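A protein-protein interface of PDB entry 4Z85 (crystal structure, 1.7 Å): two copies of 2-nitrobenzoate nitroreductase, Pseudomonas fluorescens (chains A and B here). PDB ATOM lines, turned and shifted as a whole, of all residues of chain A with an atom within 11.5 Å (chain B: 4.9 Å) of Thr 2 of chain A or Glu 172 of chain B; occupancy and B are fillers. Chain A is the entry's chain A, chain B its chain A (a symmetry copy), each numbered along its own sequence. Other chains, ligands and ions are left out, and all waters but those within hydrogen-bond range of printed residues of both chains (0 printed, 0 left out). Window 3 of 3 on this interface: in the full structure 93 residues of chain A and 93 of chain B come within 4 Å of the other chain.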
ATOM      1  N   THR A   2      17.968  22.224  -6.053  1.00  0.00           N
ATOM      2  CA  THR A   2      18.257  22.426  -7.471  1.00  0.00           C
ATOM      3  C   THR A   2      18.825  21.153  -8.097  1.00  0.00           C
ATOM      4  O   THR A   2      19.718  20.524  -7.527  1.00  0.00           O
ATOM      5  CB  THR A   2      19.247  23.593  -7.677  1.00  0.00           C
ATOM      6  OG1 THR A   2      18.698  24.788  -7.109  1.00  0.00           O
ATOM      7  CG2 THR A   2      19.532  23.824  -9.157  1.00  0.00           C
ATOM      8  N   HIS A   3      18.290  20.772  -9.255  1.00  0.00           N
ATOM      9  CA  HIS A   3      18.797  19.626 -10.011  1.00  0.00           C
ATOM     10  C   HIS A   3      19.424  20.069 -11.328  1.00  0.00           C
ATOM     11  O   HIS A   3      18.869  20.908 -12.039  1.00  0.00           O
ATOM     12  CB  HIS A   3      17.683  18.619 -10.308  1.00  0.00           C
ATOM     13  CG  HIS A   3      17.377  17.687  -9.179  1.00  0.00           C
ATOM     14  ND1 HIS A   3      16.616  18.056  -8.091  1.00  0.00           N
ATOM     15  CD2 HIS A   3      17.726  16.395  -8.971  1.00  0.00           C
ATOM     16  CE1 HIS A   3      16.502  17.032  -7.265  1.00  0.00           C
ATOM     17  NE2 HIS A   3      17.172  16.011  -7.774  1.00  0.00           N
ATOM     18  N   ILE A   4      20.580  19.500 -11.657  1.00  0.00           N
ATOM     19  CA  ILE A   4      21.220  19.763 -12.939  1.00  0.00           C
ATOM     20  C   ILE A   4      21.622  18.461 -13.615  1.00  0.00           C
ATOM     21  O   ILE A   4      22.391  17.685 -13.051  1.00  0.00           O
ATOM     22  CB  ILE A   4      22.472  20.636 -12.786  1.00  0.00           C
ATOM     23  CG1 ILE A   4      22.114  22.008 -12.202  1.00  0.00           C
ATOM     24  CG2 ILE A   4      23.178  20.769 -14.118  1.00  0.00           C
ATOM     25  CD1 ILE A   4      23.296  22.941 -12.095  1.00  0.00           C
ATOM     26  N   ALA A   5      21.104  18.222 -14.820  1.00  0.00           N
ATOM     27  CA  ALA A   5      21.476  17.035 -15.587  1.00  0.00           C
ATOM     28  C   ALA A   5      22.831  17.232 -16.270  1.00  0.00           C
ATOM     29  O   ALA A   5      23.158  18.329 -16.714  1.00  0.00           O
ATOM     30  CB  ALA A   5      20.399  16.703 -16.628  1.00  0.00           C
ATOM     31  N   MET A   6      23.624  16.166 -16.352  1.00  0.00           N
ATOM     32  CA  MET A   6      24.945  16.264 -16.959  1.00  0.00           C
ATOM     33  C   MET A   6      24.876  16.320 -18.494  1.00  0.00           C
ATOM     34  O   MET A   6      25.800  16.797 -19.156  1.00  0.00           O
ATOM     35  CB  MET A   6      25.823  15.080 -16.522  1.00  0.00           C
ATOM     36  CG  MET A   6      26.146  15.052 -15.028  1.00  0.00           C
ATOM     37  SD  MET A   6      27.154  16.449 -14.487  1.00  0.00           S
ATOM     38  CE  MET A   6      25.894  17.510 -13.783  1.00  0.00           C
ATOM     39  N   GLY A   8      23.160  18.128 -20.439  1.00  0.00           N
ATOM     40  CA  GLY A   8      23.083  19.451 -21.026  1.00  0.00           C
ATOM     41  C   GLY A   8      24.398  20.213 -21.119  1.00  0.00           C
ATOM     42  O   GLY A   8      24.447  21.281 -21.736  1.00  0.00           O
ATOM     43  N   LEU A   9      25.474  19.657 -20.563  1.00  0.00           N
ATOM     44  CA  LEU A   9      26.672  20.452 -20.289  1.00  0.00           C
ATOM     45  C   LEU A   9      27.866  20.219 -21.207  1.00  0.00           C
ATOM     46  O   LEU A   9      28.019  19.150 -21.801  1.00  0.00           O
ATOM     47  CB  LEU A   9      27.118  20.193 -18.843  1.00  0.00           C
ATOM     48  CG  LEU A   9      26.000  20.282 -17.804  1.00  0.00           C
ATOM     49  CD1 LEU A   9      26.549  19.988 -16.404  1.00  0.00           C
ATOM     50  CD2 LEU A   9      25.331  21.648 -17.838  1.00  0.00           C
ATOM     51  N   GLN A  13      31.943  22.646 -18.193  1.00  0.00           N
ATOM     52  CA  GLN A  13      30.900  22.801 -17.191  1.00  0.00           C
ATOM     53  C   GLN A  13      30.871  21.579 -16.265  1.00  0.00           C
ATOM     54  O   GLN A  13      30.756  21.709 -15.034  1.00  0.00           O
ATOM     55  CB  GLN A  13      29.544  23.021 -17.861  1.00  0.00           C
ATOM     56  CG  GLN A  13      29.463  24.376 -18.578  1.00  0.00           C
ATOM     57  CD  GLN A  13      28.187  24.546 -19.392  1.00  0.00           C
ATOM     58  OE1 GLN A  13      27.578  23.575 -19.844  1.00  0.00           O
ATOM     59  NE2 GLN A  13      27.774  25.798 -19.573  1.00  0.00           N
ATOM     60  N   TRP A  16      33.797  21.793 -13.928  1.00  0.00           N
ATOM     61  CA  TRP A  16      33.598  22.685 -12.789  1.00  0.00           C
ATOM     62  C   TRP A  16      32.623  22.133 -11.762  1.00  0.00           C
ATOM     63  O   TRP A  16      32.853  22.295 -10.555  1.00  0.00           O
ATOM     64  CB  TRP A  16      33.152  24.077 -13.252  1.00  0.00           C
ATOM     65  CG  TRP A  16      34.322  24.875 -13.687  1.00  0.00           C
ATOM     66  CD1 TRP A  16      34.768  25.049 -14.959  1.00  0.00           C
ATOM     67  CD2 TRP A  16      35.234  25.580 -12.841  1.00  0.00           C
ATOM     68  NE1 TRP A  16      35.898  25.831 -14.965  1.00  0.00           N
ATOM     69  CE2 TRP A  16      36.205  26.169 -13.675  1.00  0.00           C
ATOM     70  CE3 TRP A  16      35.318  25.777 -11.457  1.00  0.00           C
ATOM     71  CZ2 TRP A  16      37.254  26.944 -13.171  1.00  0.00           C
ATOM     72  CZ3 TRP A  16      36.360  26.550 -10.957  1.00  0.00           C
ATOM     73  CH2 TRP A  16      37.315  27.119 -11.814  1.00  0.00           C
ATOM     74  N   LEU A  17      31.554  21.472 -12.207  1.00  0.00           N
ATOM     75  CA  LEU A  17      30.570  20.966 -11.249  1.00  0.00           C
ATOM     76  C   LEU A  17      31.119  19.757 -10.450  1.00  0.00           C
ATOM     77  O   LEU A  17      30.902  19.638  -9.220  1.00  0.00           O
ATOM     78  CB  LEU A  17      29.272  20.589 -11.951  1.00  0.00           C
ATOM     79  CG  LEU A  17      28.469  21.782 -12.491  1.00  0.00           C
ATOM     80  CD1 LEU A  17      27.194  21.290 -13.159  1.00  0.00           C
ATOM     81  CD2 LEU A  17      28.143  22.761 -11.372  1.00  0.00           C
ATOM     82  N   SER A  21      32.160  19.839  -6.462  1.00  0.00           N
ATOM     83  CA  SER A  21      31.292  19.096  -5.545  1.00  0.00           C
ATOM     84  C   SER A  21      31.931  17.882  -4.841  1.00  0.00           C
ATOM     85  O   SER A  21      31.324  17.319  -3.922  1.00  0.00           O
ATOM     86  CB  SER A  21      30.026  18.635  -6.278  1.00  0.00           C
ATOM     87  OG  SER A  21      30.370  17.841  -7.399  1.00  0.00           O
ATOM     88  N   MET B 163      23.088  16.031 -10.898  1.00  0.00           N
ATOM     89  CA  MET B 163      23.441  16.479  -9.551  1.00  0.00           C
ATOM     90  C   MET B 163      22.323  17.262  -8.863  1.00  0.00           C
ATOM     91  O   MET B 163      21.651  18.083  -9.490  1.00  0.00           O
ATOM     92  CB  MET B 163      24.696  17.346  -9.591  1.00  0.00           C
ATOM     93  CG  MET B 163      25.951  16.664 -10.131  1.00  0.00           C
ATOM     94  SD  MET B 163      27.386  17.742  -9.924  1.00  0.00           S
ATOM     95  CE  MET B 163      28.683  16.818 -10.775  1.00  0.00           C
ATOM     96  N   TYR B 164      22.140  16.997  -7.574  1.00  0.00           N
ATOM     97  CA  TYR B 164      21.309  17.816  -6.696  1.00  0.00           C
ATOM     98  C   TYR B 164      22.176  18.749  -5.854  1.00  0.00           C
ATOM     99  O   TYR B 164      23.169  18.317  -5.275  1.00  0.00           O
ATOM    100  CB  TYR B 164      20.467  16.946  -5.770  1.00  0.00           C
ATOM    101  CG  TYR B 164      19.985  17.697  -4.551  1.00  0.00           C
ATOM    102  CD1 TYR B 164      18.887  18.547  -4.627  1.00  0.00           C
ATOM    103  CD2 TYR B 164      20.638  17.578  -3.329  1.00  0.00           C
ATOM    104  CE1 TYR B 164      18.448  19.244  -3.525  1.00  0.00           C
ATOM    105  CE2 TYR B 164      20.206  18.279  -2.217  1.00  0.00           C
ATOM    106  CZ  TYR B 164      19.108  19.107  -2.323  1.00  0.00           C
ATOM    107  OH  TYR B 164      18.671  19.799  -1.223  1.00  0.00           O
ATOM    108  N   PHE B 165      21.790  20.019  -5.773  1.00  0.00           N
ATOM    109  CA  PHE B 165      22.430  20.977  -4.865  1.00  0.00           C
ATOM    110  C   PHE B 165      21.383  21.661  -3.988  1.00  0.00           C
ATOM    111  O   PHE B 165      20.322  22.028  -4.492  1.00  0.00           O
ATOM    112  CB  PHE B 165      23.177  22.076  -5.623  1.00  0.00           C
ATOM    113  CG  PHE B 165      24.132  21.586  -6.662  1.00  0.00           C
ATOM    114  CD1 PHE B 165      23.687  21.264  -7.934  1.00  0.00           C
ATOM    115  CD2 PHE B 165      25.493  21.507  -6.389  1.00  0.00           C
ATOM    116  CE1 PHE B 165      24.574  20.832  -8.904  1.00  0.00           C
ATOM    117  CE2 PHE B 165      26.382  21.080  -7.362  1.00  0.00           C
ATOM    118  CZ  PHE B 165      25.925  20.744  -8.614  1.00  0.00           C
ATOM    119  N   GLU B 167      19.941  24.910  -2.739  1.00  0.00           N
ATOM    120  CA  GLU B 167      19.926  26.083  -3.611  1.00  0.00           C
ATOM    121  C   GLU B 167      21.024  27.086  -3.282  1.00  0.00           C
ATOM    122  O   GLU B 167      21.594  27.704  -4.177  1.00  0.00           O
ATOM    123  CB  GLU B 167      18.562  26.774  -3.559  1.00  0.00           C
ATOM    124  CG  GLU B 167      17.939  26.948  -4.924  1.00  0.00           C
ATOM    125  CD  GLU B 167      16.524  27.475  -4.851  1.00  0.00           C
ATOM    126  OE1 GLU B 167      16.293  28.446  -4.096  1.00  0.00           O
ATOM    127  OE2 GLU B 167      15.645  26.912  -5.544  1.00  0.00           O
ATOM    128  N   ILE B 170      24.686  26.550  -5.094  1.00  0.00           N
ATOM    129  CA  ILE B 170      24.882  26.506  -6.537  1.00  0.00           C
ATOM    130  C   ILE B 170      24.520  27.833  -7.190  1.00  0.00           C
ATOM    131  O   ILE B 170      23.482  28.426  -6.891  1.00  0.00           O
ATOM    132  CB  ILE B 170      24.053  25.350  -7.177  1.00  0.00           C
ATOM    133  CG1 ILE B 170      24.227  25.308  -8.698  1.00  0.00           C
ATOM    134  CG2 ILE B 170      22.576  25.442  -6.794  1.00  0.00           C
ATOM    135  CD1 ILE B 170      25.613  24.870  -9.164  1.00  0.00           C
ATOM    136  N   ASP B 171      25.409  28.311  -8.052  1.00  0.00           N
ATOM    137  CA  ASP B 171      25.126  29.458  -8.903  1.00  0.00           C
ATOM    138  C   ASP B 171      24.588  28.917 -10.228  1.00  0.00           C
ATOM    139  O   ASP B 171      25.350  28.663 -11.161  1.00  0.00           O
ATOM    140  CB  ASP B 171      26.388  30.303  -9.107  1.00  0.00           C
ATOM    141  CG  ASP B 171      26.118  31.606  -9.845  1.00  0.00           C
ATOM    142  OD1 ASP B 171      25.065  31.722 -10.509  1.00  0.00           O
ATOM    143  OD2 ASP B 171      26.974  32.514  -9.762  1.00  0.00           O
ATOM    144  N   GLU B 172      23.274  28.736 -10.292  1.00  0.00           N
ATOM    145  CA  GLU B 172      22.640  28.054 -11.418  1.00  0.00           C
ATOM    146  C   GLU B 172      22.863  28.782 -12.744  1.00  0.00           C
ATOM    147  O   GLU B 172      23.010  28.147 -13.791  1.00  0.00           O
ATOM    148  CB  GLU B 172      21.143  27.885 -11.155  1.00  0.00           C
ATOM    149  CG  GLU B 172      20.412  27.100 -12.231  1.00  0.00           C
ATOM    150  CD  GLU B 172      18.931  26.953 -11.942  1.00  0.00           C
ATOM    151  OE1 GLU B 172      18.240  27.990 -11.829  1.00  0.00           O
ATOM    152  OE2 GLU B 172      18.456  25.800 -11.834  1.00  0.00           O
ATOM    153  N   GLU B 173      22.904  30.110 -12.704  1.00  0.00           N
ATOM    154  CA  GLU B 173      23.149  30.877 -13.917  1.00  0.00           C
ATOM    155  C   GLU B 173      24.573  30.679 -14.417  1.00  0.00           C
ATOM    156  O   GLU B 173      24.811  30.619 -15.624  1.00  0.00           O
ATOM    157  CB  GLU B 173      22.874  32.364 -13.689  1.00  0.00           C
ATOM    158  CG  GLU B 173      21.430  32.766 -13.961  1.00  0.00           C
ATOM    159  CD  GLU B 173      21.161  34.232 -13.678  1.00  0.00           C
ATOM    160  OE1 GLU B 173      22.073  35.059 -13.897  1.00  0.00           O
ATOM    161  OE2 GLU B 173      20.037  34.557 -13.240  1.00  0.00           O
ATOM    162  N   LYS B 174      25.520  30.570 -13.490  1.00  0.00           N
ATOM    163  CA  LYS B 174      26.924  30.445 -13.866  1.00  0.00           C
ATOM    164  C   LYS B 174      27.344  28.981 -14.021  1.00  0.00           C
ATOM    165  O   LYS B 174      28.403  28.693 -14.575  1.00  0.00           O
ATOM    166  CB  LYS B 174      27.811  31.144 -12.831  1.00  0.00           C
ATOM    167  CG  LYS B 174      29.210  31.489 -13.332  1.00  0.00           C
ATOM    168  CD  LYS B 174      29.851  32.600 -12.504  1.00  0.00           C
ATOM    169  CE  LYS B 174      31.116  32.117 -11.808  1.00  0.00           C
ATOM    170  NZ  LYS B 174      31.821  33.217 -11.086  1.00  0.00           N
ATOM    171  N   LEU B 175      26.494  28.073 -13.547  1.00  0.00           N
ATOM    172  CA  LEU B 175      26.822  26.646 -13.461  1.00  0.00           C
ATOM    173  C   LEU B 175      28.101  26.438 -12.664  1.00  0.00           C
ATOM    174  O   LEU B 175      29.012  25.733 -13.098  1.00  0.00           O
ATOM    175  CB  LEU B 175      26.953  26.026 -14.852  1.00  0.00           C
ATOM    176  CG  LEU B 175      25.621  25.872 -15.577  1.00  0.00           C
ATOM    177  CD1 LEU B 175      25.816  25.221 -16.935  1.00  0.00           C
ATOM    178  CD2 LEU B 175      24.669  25.062 -14.721  1.00  0.00           C
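Among the printed residues, pairs that only touch across the chains: Thr 2 of chain A with Glu 167 of chain B (3.2 Å), Thr 2 of chain A with Tyr 164 of chain B (3.2 Å), His 3 of chain A with Met 163 of chain B (3.3 Å), Gln 13 of chain A with Leu 175 of chain B (3.3 Å), Thr 2 of chain A with Glu 172 of chain B (3.5 Å), Leu 17 of chain A with Leu 175 of chain B (3.5 Å), Ile 4 of chain A with Leu 175 of chain B (3.6 Å), Thr 2 of chain A with Met 163 of chain B (3.7 Å), Leu 9 of chain A with Leu 175 of chain B (3.7 Å), Met 6 of chain A with Met 163 of chain B (3.7 Å), Leu 17 of chain A with Met 163 of chain B (3.8 Å), His 3 of chain A with Tyr 164 of chain B (3.9 Å), Thr 2 of chain A with Ile 170 of chain B (3.9 Å), Ser 21 of chain A with Met 163 of chain B (3.9 Å) and Leu 17 of chain A with Ile 170 of chain B (3.97 Å).
N of Phe 165 of chain B sits at hydrogen-bond distance from O of Thr 2 of chain A (2.8 Å). The backbone NH of Ile 4 of chain A sits at hydrogen-bond distance from the backbone carbonyl oxygen of Met 163 of chain B, at 2.8 Å.
Thr 2 of chain A touches just these residues of chain B: Met 163 (3.7 Å), Tyr 164 (3.2 Å), Phe 165 (2.8 Å), Glu 167 (3.2 Å), Ile 170 (3.9 Å) and Glu 172 (3.5 Å). Of the printed residues of chain B, His 3 of chain A touches Met 163 and Tyr 164. Gly 8 of chain A touches none of the printed residues of chain B. Of the printed residues of chain B, Leu 9 of chain A touches Leu 175. Of the printed residues of chain B, Leu 17 of chain A touches Met 163, Ile 170 and Leu 175. Of the printed residues of chain B, Ser 21 of chain A touches Met 163 (3.9 Å). Of the printed residues of chain A, Met 163 of chain B touches Thr 2, His 3, Ile 4, Met 6, Leu 17 and Ser 21. Of chain A, only Thr 2 (2.8 Å) comes within 4 Å of Phe 165 of chain B. Of chain A, only Thr 2 comes within 4 Å of Glu 167 of chain B. No residue of chain A comes within 4 Å of Asp 171 of chain B. Glu 172 of chain B touches just one residue of chain A: Thr 2. No residue of chain A comes within 4 Å of Glu 173 of chain B. Lys 174 of chain B touches none of the printed residues of chain A. Of chain A, only Ile 4, Leu 9, Gln 13 and Leu 17 come within 4 Å of Leu 175 of chain B. The nearest printed residue of chain B that does not touch Gln 13 of chain A is Lys 174 of chain B (5.8 Å).
No position is printed for both chains. Of the 17 pairs that touch across the chains among the printed residues, none has its exchanged pair printed and touching as well.
Hydrophobic or aromatic side chains of chain B that line the printed part of chain A: Met 163, Tyr 164, Ile 170 and Leu 175. Printed residues of chain A that touch a printed residue of chain B: Thr 2, His 3, Ile 4, Met 6, Leu 9, Gln 13, Leu 17 and Ser 21. Among the printed residues, 17 pairs touch across the chains. Among the printed residues, no Asp or Glu carboxylate lies within 4 Å of a Lys or Arg side-chain nitrogen of the other chain.
O of Leu 17 of chain A sits at hydrogen-bond distance from OG of Ser 21 of chain A (2.6 Å).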
